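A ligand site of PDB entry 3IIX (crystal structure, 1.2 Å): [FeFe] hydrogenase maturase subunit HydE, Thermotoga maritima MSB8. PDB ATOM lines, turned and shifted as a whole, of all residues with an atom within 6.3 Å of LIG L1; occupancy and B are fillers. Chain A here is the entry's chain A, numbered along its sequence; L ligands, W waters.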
ATOM      1  N   CYS A  63      15.531  14.432 -16.864  1.00  0.00           N
ATOM      2  CA  CYS A  63      16.389  15.173 -17.780  1.00  0.00           C
ATOM      3  C   CYS A  63      15.899  16.588 -18.011  1.00  0.00           C
ATOM      4  O   CYS A  63      14.703  16.827 -18.215  1.00  0.00           O
ATOM      5  CB  CYS A  63      16.546  14.448 -19.131  1.00  0.00           C
ATOM      6  SG  CYS A  63      17.987  15.155 -20.041  1.00  0.00           S
ATOM      7  N   CYS A  67      16.182  16.531 -26.295  1.00  0.00           N
ATOM      8  CA  CYS A  67      16.631  15.914 -27.559  1.00  0.00           C
ATOM      9  C   CYS A  67      15.451  15.243 -28.249  1.00  0.00           C
ATOM     10  O   CYS A  67      14.661  14.540 -27.618  1.00  0.00           O
ATOM     11  CB  CYS A  67      17.727  14.876 -27.241  1.00  0.00           C
ATOM     12  SG  CYS A  67      19.132  15.565 -26.315  1.00  0.00           S
ATOM     13  N   TYR A  69      15.018  12.820 -30.272  1.00  0.00           N
ATOM     14  CA  TYR A  69      14.982  11.352 -30.469  1.00  0.00           C
ATOM     15  C   TYR A  69      14.722  10.580 -29.182  1.00  0.00           C
ATOM     16  O   TYR A  69      14.381   9.402 -29.247  1.00  0.00           O
ATOM     17  CB  TYR A  69      16.334  10.859 -31.024  1.00  0.00           C
ATOM     18  CG  TYR A  69      17.565  11.479 -30.416  1.00  0.00           C
ATOM     19  CD1 TYR A  69      18.065  11.019 -29.200  1.00  0.00           C
ATOM     20  CD2 TYR A  69      18.223  12.543 -31.028  1.00  0.00           C
ATOM     21  CE1 TYR A  69      19.193  11.576 -28.633  1.00  0.00           C
ATOM     22  CE2 TYR A  69      19.351  13.101 -30.461  1.00  0.00           C
ATOM     23  CZ  TYR A  69      19.821  12.610 -29.248  1.00  0.00           C
ATOM     24  OH  TYR A  69      20.938  13.214 -28.720  1.00  0.00           O
ATOM     25  N   CYS A  70      14.836  11.229 -28.033  1.00  0.00           N
ATOM     26  CA  CYS A  70      15.015  10.527 -26.743  1.00  0.00           C
ATOM     27  C   CYS A  70      13.727  10.435 -25.946  1.00  0.00           C
ATOM     28  O   CYS A  70      13.094  11.448 -25.672  1.00  0.00           O
ATOM     29  CB  CYS A  70      16.096  11.197 -25.880  1.00  0.00           C
ATOM     30  SG  CYS A  70      16.421  10.334 -24.374  1.00  0.00           S
ATOM     31  N   LEU A  72      13.447  10.172 -22.834  1.00  0.00           N
ATOM     32  CA  LEU A  72      13.556  10.868 -21.541  1.00  0.00           C
ATOM     33  C   LEU A  72      13.466  12.374 -21.694  1.00  0.00           C
ATOM     34  O   LEU A  72      13.603  13.091 -20.714  1.00  0.00           O
ATOM     35  CB  LEU A  72      14.858  10.522 -20.769  1.00  0.00           C
ATOM     36  CG  LEU A  72      15.175   9.027 -20.690  1.00  0.00           C
ATOM     37  CD1 LEU A  72      16.408   8.847 -19.790  1.00  0.00           C
ATOM     38  CD2 LEU A  72      14.007   8.175 -20.248  1.00  0.00           C
ATOM     39  N   GLN A 107      24.839   5.952 -15.586  1.00  0.00           N
ATOM     40  CA  GLN A 107      24.223   6.741 -16.645  1.00  0.00           C
ATOM     41  C   GLN A 107      22.904   7.320 -16.155  1.00  0.00           C
ATOM     42  O   GLN A 107      22.186   6.691 -15.397  1.00  0.00           O
ATOM     43  CB  GLN A 107      23.983   5.933 -17.921  1.00  0.00           C
ATOM     44  CG  GLN A 107      23.613   6.759 -19.160  1.00  0.00           C
ATOM     45  CD  GLN A 107      23.314   5.918 -20.349  1.00  0.00           C
ATOM     46  OE1 GLN A 107      22.220   5.364 -20.488  1.00  0.00           O
ATOM     47  NE2 GLN A 107      24.290   5.801 -21.224  1.00  0.00           N
ATOM     48  N   SER A 108      22.588   8.509 -16.620  1.00  0.00           N
ATOM     49  CA  SER A 108      21.355   9.149 -16.264  1.00  0.00           C
ATOM     50  C   SER A 108      20.952  10.140 -17.351  1.00  0.00           C
ATOM     51  O   SER A 108      21.754  10.538 -18.217  1.00  0.00           O
ATOM     52  CB  SER A 108      21.476   9.859 -14.933  1.00  0.00           C
ATOM     53  OG  SER A 108      22.449  10.889 -14.982  1.00  0.00           O
ATOM     54  N   GLY A 109      19.698  10.602 -17.261  1.00  0.00           N
ATOM     55  CA  GLY A 109      19.383  11.883 -17.902  1.00  0.00           C
ATOM     56  C   GLY A 109      20.220  12.976 -17.270  1.00  0.00           C
ATOM     57  O   GLY A 109      20.864  12.776 -16.242  1.00  0.00           O
ATOM     58  N   GLU A 110      20.209  14.148 -17.884  1.00  0.00           N
ATOM     59  CA  GLU A 110      20.886  15.305 -17.277  1.00  0.00           C
ATOM     60  C   GLU A 110      20.029  15.823 -16.137  1.00  0.00           C
ATOM     61  O   GLU A 110      19.233  16.770 -16.283  1.00  0.00           O
ATOM     62  CB  GLU A 110      21.161  16.402 -18.306  1.00  0.00           C
ATOM     63  CG  GLU A 110      22.185  15.997 -19.358  1.00  0.00           C
ATOM     64  CD  GLU A 110      22.727  17.177 -20.134  1.00  0.00           C
ATOM     65  OE1 GLU A 110      22.367  18.332 -19.798  1.00  0.00           O
ATOM     66  OE2 GLU A 110      23.512  16.981 -21.095  1.00  0.00           O
ATOM     67  N   SER A 136      28.334   8.575 -17.509  1.00  0.00           N
ATOM     68  CA  SER A 136      27.681   8.940 -18.738  1.00  0.00           C
ATOM     69  C   SER A 136      26.487   9.817 -18.344  1.00  0.00           C
ATOM     70  O   SER A 136      25.345   9.368 -18.292  1.00  0.00           O
ATOM     71  CB  SER A 136      27.225   7.690 -19.486  1.00  0.00           C
ATOM     72  OG  SER A 136      26.602   7.954 -20.720  1.00  0.00           O
ATOM     73  N   LEU A 137      26.793  11.074 -18.060  1.00  0.00           N
ATOM     74  CA  LEU A 137      25.838  11.992 -17.413  1.00  0.00           C
ATOM     75  C   LEU A 137      25.504  13.197 -18.275  1.00  0.00           C
ATOM     76  O   LEU A 137      24.732  14.062 -17.866  1.00  0.00           O
ATOM     77  CB  LEU A 137      26.397  12.482 -16.066  1.00  0.00           C
ATOM     78  CG  LEU A 137      26.923  11.413 -15.107  1.00  0.00           C
ATOM     79  CD1 LEU A 137      27.464  12.040 -13.821  1.00  0.00           C
ATOM     80  CD2 LEU A 137      25.868  10.329 -14.850  1.00  0.00           C
ATOM     81  N   GLY A 138      26.051  13.261 -19.491  1.00  0.00           N
ATOM     82  CA  GLY A 138      25.742  14.356 -20.388  1.00  0.00           C
ATOM     83  C   GLY A 138      26.739  15.511 -20.257  1.00  0.00           C
ATOM     84  O   GLY A 138      27.895  15.343 -19.828  1.00  0.00           O
ATOM     85  N   GLU A 139      26.269  16.704 -20.645  1.00  0.00           N
ATOM     86  CA  GLU A 139      27.073  17.928 -20.732  1.00  0.00           C
ATOM     87  C   GLU A 139      26.977  18.742 -19.454  1.00  0.00           C
ATOM     88  O   GLU A 139      25.905  19.136 -19.057  1.00  0.00           O
ATOM     89  CB  GLU A 139      26.547  18.769 -21.884  1.00  0.00           C
ATOM     90  CG  GLU A 139      26.699  18.101 -23.244  1.00  0.00           C
ATOM     91  CD  GLU A 139      25.978  18.793 -24.380  1.00  0.00           C
ATOM     92  OE1 GLU A 139      25.935  20.043 -24.387  1.00  0.00           O
ATOM     93  OE2 GLU A 139      25.466  18.069 -25.268  1.00  0.00           O
ATOM     94  N   LEU A 157      31.570   8.507 -21.026  1.00  0.00           N
ATOM     95  CA  LEU A 157      30.900   8.261 -22.303  1.00  0.00           C
ATOM     96  C   LEU A 157      30.038   9.450 -22.655  1.00  0.00           C
ATOM     97  O   LEU A 157      29.111   9.789 -21.929  1.00  0.00           O
ATOM     98  CB  LEU A 157      30.009   7.017 -22.248  1.00  0.00           C
ATOM     99  CG  LEU A 157      30.666   5.767 -21.696  1.00  0.00           C
ATOM    100  CD1 LEU A 157      29.635   4.624 -21.580  1.00  0.00           C
ATOM    101  CD2 LEU A 157      31.885   5.386 -22.575  1.00  0.00           C
ATOM    102  N   LEU A 158      30.299  10.046 -23.823  1.00  0.00           N
ATOM    103  CA  LEU A 158      29.535  11.204 -24.303  1.00  0.00           C
ATOM    104  C   LEU A 158      29.444  11.079 -25.814  1.00  0.00           C
ATOM    105  O   LEU A 158      30.281  11.625 -26.532  1.00  0.00           O
ATOM    106  CB  LEU A 158      30.200  12.500 -23.911  1.00  0.00           C
ATOM    107  CG  LEU A 158      29.362  13.767 -24.036  1.00  0.00           C
ATOM    108  CD1 LEU A 158      28.245  13.816 -23.006  1.00  0.00           C
ATOM    109  CD2 LEU A 158      30.280  15.033 -23.906  1.00  0.00           C
ATOM    110  N   ARG A 159      28.490  10.308 -26.312  1.00  0.00           N
ATOM    111  CA  ARG A 159      28.390  10.104 -27.753  1.00  0.00           C
ATOM    112  C   ARG A 159      28.271  11.453 -28.429  1.00  0.00           C
ATOM    113  O   ARG A 159      27.556  12.315 -27.969  1.00  0.00           O
ATOM    114  CB  ARG A 159      27.182   9.266 -28.093  1.00  0.00           C
ATOM    115  CG  ARG A 159      27.305   7.835 -27.677  1.00  0.00           C
ATOM    116  CD  ARG A 159      26.220   7.083 -28.325  1.00  0.00           C
ATOM    117  NE  ARG A 159      26.131   5.734 -27.837  1.00  0.00           N
ATOM    118  CZ  ARG A 159      25.220   4.883 -28.279  1.00  0.00           C
ATOM    119  NH1 ARG A 159      24.337   5.268 -29.192  1.00  0.00           N
ATOM    120  NH2 ARG A 159      25.172   3.664 -27.787  1.00  0.00           N
ATOM    121  N   GLU A 161      26.853  11.863 -31.235  1.00  0.00           N
ATOM    122  CA  GLU A 161      25.478  11.751 -31.771  1.00  0.00           C
ATOM    123  C   GLU A 161      25.412  11.893 -33.287  1.00  0.00           C
ATOM    124  O   GLU A 161      24.958  10.997 -33.982  1.00  0.00           O
ATOM    125  CB  GLU A 161      24.501  12.706 -31.084  1.00  0.00           C
ATOM    126  CG  GLU A 161      24.498  12.652 -29.555  1.00  0.00           C
ATOM    127  CD  GLU A 161      24.168  11.318 -28.941  1.00  0.00           C
ATOM    128  OE1 GLU A 161      24.007  10.301 -29.646  1.00  0.00           O
ATOM    129  OE2 GLU A 161      24.107  11.285 -27.684  1.00  0.00           O
ATOM    130  N   ARG A 172      19.088  18.431 -31.100  1.00  0.00           N
ATOM    131  CA  ARG A 172      19.506  18.646 -29.722  1.00  0.00           C
ATOM    132  C   ARG A 172      19.426  20.152 -29.467  1.00  0.00           C
ATOM    133  O   ARG A 172      20.457  20.859 -29.401  1.00  0.00           O
ATOM    134  CB  ARG A 172      20.895  18.072 -29.518  1.00  0.00           C
ATOM    135  CG  ARG A 172      21.007  16.621 -29.998  1.00  0.00           C
ATOM    136  CD  ARG A 172      22.282  15.936 -29.522  1.00  0.00           C
ATOM    137  NE  ARG A 172      22.258  15.781 -28.064  1.00  0.00           N
ATOM    138  CZ  ARG A 172      23.035  16.403 -27.201  1.00  0.00           C
ATOM    139  NH1 ARG A 172      24.047  17.167 -27.602  1.00  0.00           N
ATOM    140  NH2 ARG A 172      22.797  16.261 -25.906  1.00  0.00           N
ATOM    141  N   ARG A 180      29.277  19.926 -27.708  1.00  0.00           N
ATOM    142  CA  ARG A 180      29.524  18.506 -27.502  1.00  0.00           C
ATOM    143  C   ARG A 180      30.992  18.175 -27.709  1.00  0.00           C
ATOM    144  O   ARG A 180      31.593  17.464 -26.915  1.00  0.00           O
ATOM    145  CB  ARG A 180      28.667  17.707 -28.479  1.00  0.00           C
ATOM    146  CG  ARG A 180      28.455  16.248 -28.127  1.00  0.00           C
ATOM    147  CD  ARG A 180      27.495  16.110 -26.948  1.00  0.00           C
ATOM    148  NE  ARG A 180      27.036  14.747 -26.758  1.00  0.00           N
ATOM    149  CZ  ARG A 180      26.224  14.347 -25.788  1.00  0.00           C
ATOM    150  NH1 ARG A 180      25.734  15.224 -24.919  1.00  0.00           N
ATOM    151  NH2 ARG A 180      25.883  13.070 -25.701  1.00  0.00           N
ATOM    152  N   TYR A 303      13.261   3.491 -17.938  1.00  0.00           N
ATOM    153  CA  TYR A 303      14.410   4.112 -18.623  1.00  0.00           C
ATOM    154  C   TYR A 303      14.473   3.557 -20.019  1.00  0.00           C
ATOM    155  O   TYR A 303      15.212   2.630 -20.307  1.00  0.00           O
ATOM    156  CB  TYR A 303      15.682   3.819 -17.878  1.00  0.00           C
ATOM    157  CG  TYR A 303      16.875   4.659 -18.253  1.00  0.00           C
ATOM    158  CD1 TYR A 303      17.205   5.796 -17.517  1.00  0.00           C
ATOM    159  CD2 TYR A 303      17.719   4.282 -19.285  1.00  0.00           C
ATOM    160  CE1 TYR A 303      18.340   6.527 -17.757  1.00  0.00           C
ATOM    161  CE2 TYR A 303      18.866   5.033 -19.544  1.00  0.00           C
ATOM    162  CZ  TYR A 303      19.171   6.130 -18.771  1.00  0.00           C
ATOM    163  OH  TYR A 303      20.331   6.824 -19.001  1.00  0.00           O
ATOM    164  N   LEU A 305      14.999   4.946 -23.573  1.00  0.00           N
ATOM    165  CA  LEU A 305      15.392   5.982 -24.505  1.00  0.00           C
ATOM    166  C   LEU A 305      14.699   5.746 -25.835  1.00  0.00           C
ATOM    167  O   LEU A 305      14.321   6.683 -26.528  1.00  0.00           O
ATOM    168  CB  LEU A 305      16.913   5.968 -24.695  1.00  0.00           C
ATOM    169  CG  LEU A 305      17.780   5.889 -23.437  1.00  0.00           C
ATOM    170  CD1 LEU A 305      19.249   6.087 -23.790  1.00  0.00           C
ATOM    171  CD2 LEU A 305      17.325   6.883 -22.419  1.00  0.00           C
HETATM  172  N1  LIG L   1      22.025  12.141 -21.026  1.00  0.00           N
HETATM  173  C1  LIG L   1      23.386  11.627 -21.324  1.00  0.00           C
HETATM  174  C2  LIG L   1      23.703  11.950 -22.774  1.00  0.00           C
HETATM  175  O1  LIG L   1      24.893  11.863 -23.185  1.00  0.00           O
HETATM  176  C3  LIG L   1      23.420  10.111 -21.138  1.00  0.00           C
HETATM  177  C4  LIG L   1      22.940   9.302 -22.320  1.00  0.00           C
HETATM  178  S1  LIG L   1      21.217   9.589 -22.781  1.00  0.00           S
HETATM  179  C5  LIG L   1      20.456   8.845 -21.322  1.00  0.00           C
HETATM  180  O2  LIG L   1      22.793  12.306 -23.559  1.00  0.00           O
HETATM  181 FE1  LG2 L   2      19.172  14.105 -24.509  1.00  0.00          FE
HETATM  182 FE2  LG2 L   2      20.662  12.199 -22.803  1.00  0.00          FE
HETATM  183 FE3  LG2 L   2      18.424  13.921 -21.902  1.00  0.00          FE
HETATM  184 FE4  LG2 L   2      17.900  11.887 -23.574  1.00  0.00          FE
HETATM  185  S1  LG2 L   2      18.727  11.695 -21.483  1.00  0.00           S
HETATM  186  S2  LG2 L   2      17.007  14.022 -23.670  1.00  0.00           S
HETATM  187  S3  LG2 L   2      19.757  11.915 -24.954  1.00  0.00           S
HETATM  188  S4  LG2 L   2      20.467  14.635 -22.702  1.00  0.00           S
HETATM  189  N1  LG3 L   3      17.305   5.396 -30.576  1.00  0.00           N
HETATM  190  C1  LG3 L   3      18.581   4.871 -30.508  1.00  0.00           C
HETATM  191  N2  LG3 L   3      19.505   5.366 -29.647  1.00  0.00           N
HETATM  192  C2  LG3 L   3      19.141   6.375 -28.826  1.00  0.00           C
HETATM  193  N3  LG3 L   3      19.864   7.054 -27.907  1.00  0.00           N
HETATM  194  C3  LG3 L   3      19.039   7.980 -27.324  1.00  0.00           C
HETATM  195  N4  LG3 L   3      17.810   7.894 -27.878  1.00  0.00           N
HETATM  196  C4  LG3 L   3      17.841   6.916 -28.844  1.00  0.00           C
HETATM  197  C5  LG3 L   3      16.922   6.388 -29.720  1.00  0.00           C
HETATM  198  N5  LG3 L   3      15.662   6.849 -29.813  1.00  0.00           N
HETATM  199  C6  LG3 L   3      21.306   6.856 -27.685  1.00  0.00           C
HETATM  200  C7  LG3 L   3      22.089   8.170 -27.835  1.00  0.00           C
HETATM  201  C8  LG3 L   3      22.700   8.364 -26.462  1.00  0.00           C
HETATM  202  C9  LG3 L   3      22.828   6.913 -26.016  1.00  0.00           C
HETATM  203  C10 LG3 L   3      22.939   6.678 -24.520  1.00  0.00           C
HETATM  204  O1  LG3 L   3      21.591   6.334 -26.422  1.00  0.00           O
HETATM  205  O2  LG3 L   3      23.059   7.976 -28.846  1.00  0.00           O
HETATM  206  O3  LG3 L   3      23.963   9.006 -26.453  1.00  0.00           O
HETATM  207  O   HOH W   1      25.968   9.677 -24.722  1.00  0.00           O
HETATM  208  O   HOH W   2      26.859  11.055 -21.295  1.00  0.00           O
HETATM  209  O   HOH W   3      23.689  15.185 -23.053  1.00  0.00           O
HETATM  210  O   HOH W   4      22.428  13.099 -26.452  1.00  0.00           O
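Water W2 lies within hydrogen-bond range of the backbone carbonyl oxygen (O) of Leu 157 (2.7 Å), an oxygen (O1) of LIG L1 (2.8 Å), the backbone NH (N) of Gly 138 (3.0 Å), the side-chain hydroxyl (OG) of Ser 136 (3.2 Å) and the backbone NH (N) of Leu 137 (3.2 Å). Water W1 lies within hydrogen-bond range of an oxygen (O3) of LG3 L3, an oxygen (O1) of LIG L1 and the backbone NH of Arg 159. Water W4 lies within hydrogen-bond range of the side-chain hydroxyl of Tyr 69 (2.7 Å), the side-chain carboxylate of Glu 161 (2.8 Å), the guanidinium group of Arg 172 (3.1 Å) and a sulfur (S3) of LG2 L2 (3.3 Å). Water W3 lies within hydrogen-bond range of OE2 of Glu 110, NH1 of Arg 180, NH2 of Arg 172 and S4 of LG2 L2.
NH2 of Arg 180 lies within salt-bridge range of OE2 of Glu 161 (3.2 Å). The guanidinium group of Arg 180 lies within salt-bridge range of the side-chain carboxylate of Glu 139, at 2.9 Å. The guanidinium group of Arg 180 lies within hydrogen-bond range of the backbone carbonyl oxygen of Arg 159. O of Leu 157 is in hydrogen-bond range of OG of Ser 136. The backbone NH of Ser 108 lies within hydrogen-bond range of the backbone carbonyl oxygen of Ser 136. OE1 of Gln 107 is in hydrogen-bond range of OH of Tyr 303. The side-chain hydroxyl of Ser 136 sits at hydrogen-bond distance from the side-chain amide nitrogen of Gln 107.
Residues that only touch LIG L1: Gln 107 (3.9 Å), Ser 136 (3.5 Å), Gly 138 (3.6 Å), Leu 158 (3.9 Å), Tyr 303 (3.1 Å) and Leu 305 (3.9 Å). Hydrophobic or aromatic side chains that line LIG L1: Leu 158, Tyr 303 and Leu 305. Within 4 Å of LIG L1: Gln 107, Ser 108, Ser 136, Gly 138, Leu 158, Arg 180, Tyr 303 and Leu 305. The nearest printed residue that does not touch LIG L1 is Leu 137 (4.03 Å).
An iron atom (FE1) of LG2 L2 is bound by the side-chain sulfur (SG) of Cys 67 (2.3 Å). An iron atom (FE4) of LG2 L2 is bound by the side-chain sulfur of Cys 70. S2 of LG2 L2 sits close to N of Cys 67, 3.7 Å away. The backbone carbonyl oxygen of Tyr 69 lies within hydrogen-bond range of a nitrogen (N5) of LG3 L3 (2.9 Å). The guanidinium group of Arg 180 is in salt-bridge range of an oxygen (O1) of LIG L1. OE2 of Glu 161 sits at hydrogen-bond distance from O3 of LG3 L3, 2.6 Å away. O of Ser 108 sits close to N1 of LIG L1. The guanidinium group of Arg 159 sits at hydrogen-bond distance from an oxygen (O2) of LG3 L3 (3.0 Å). SG of Cys 63 is bound to FE3 of LG2 L2 (2.3 Å).
N1 of LIG L1 binds FE2 of LG2 L2, 2.2 Å away.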
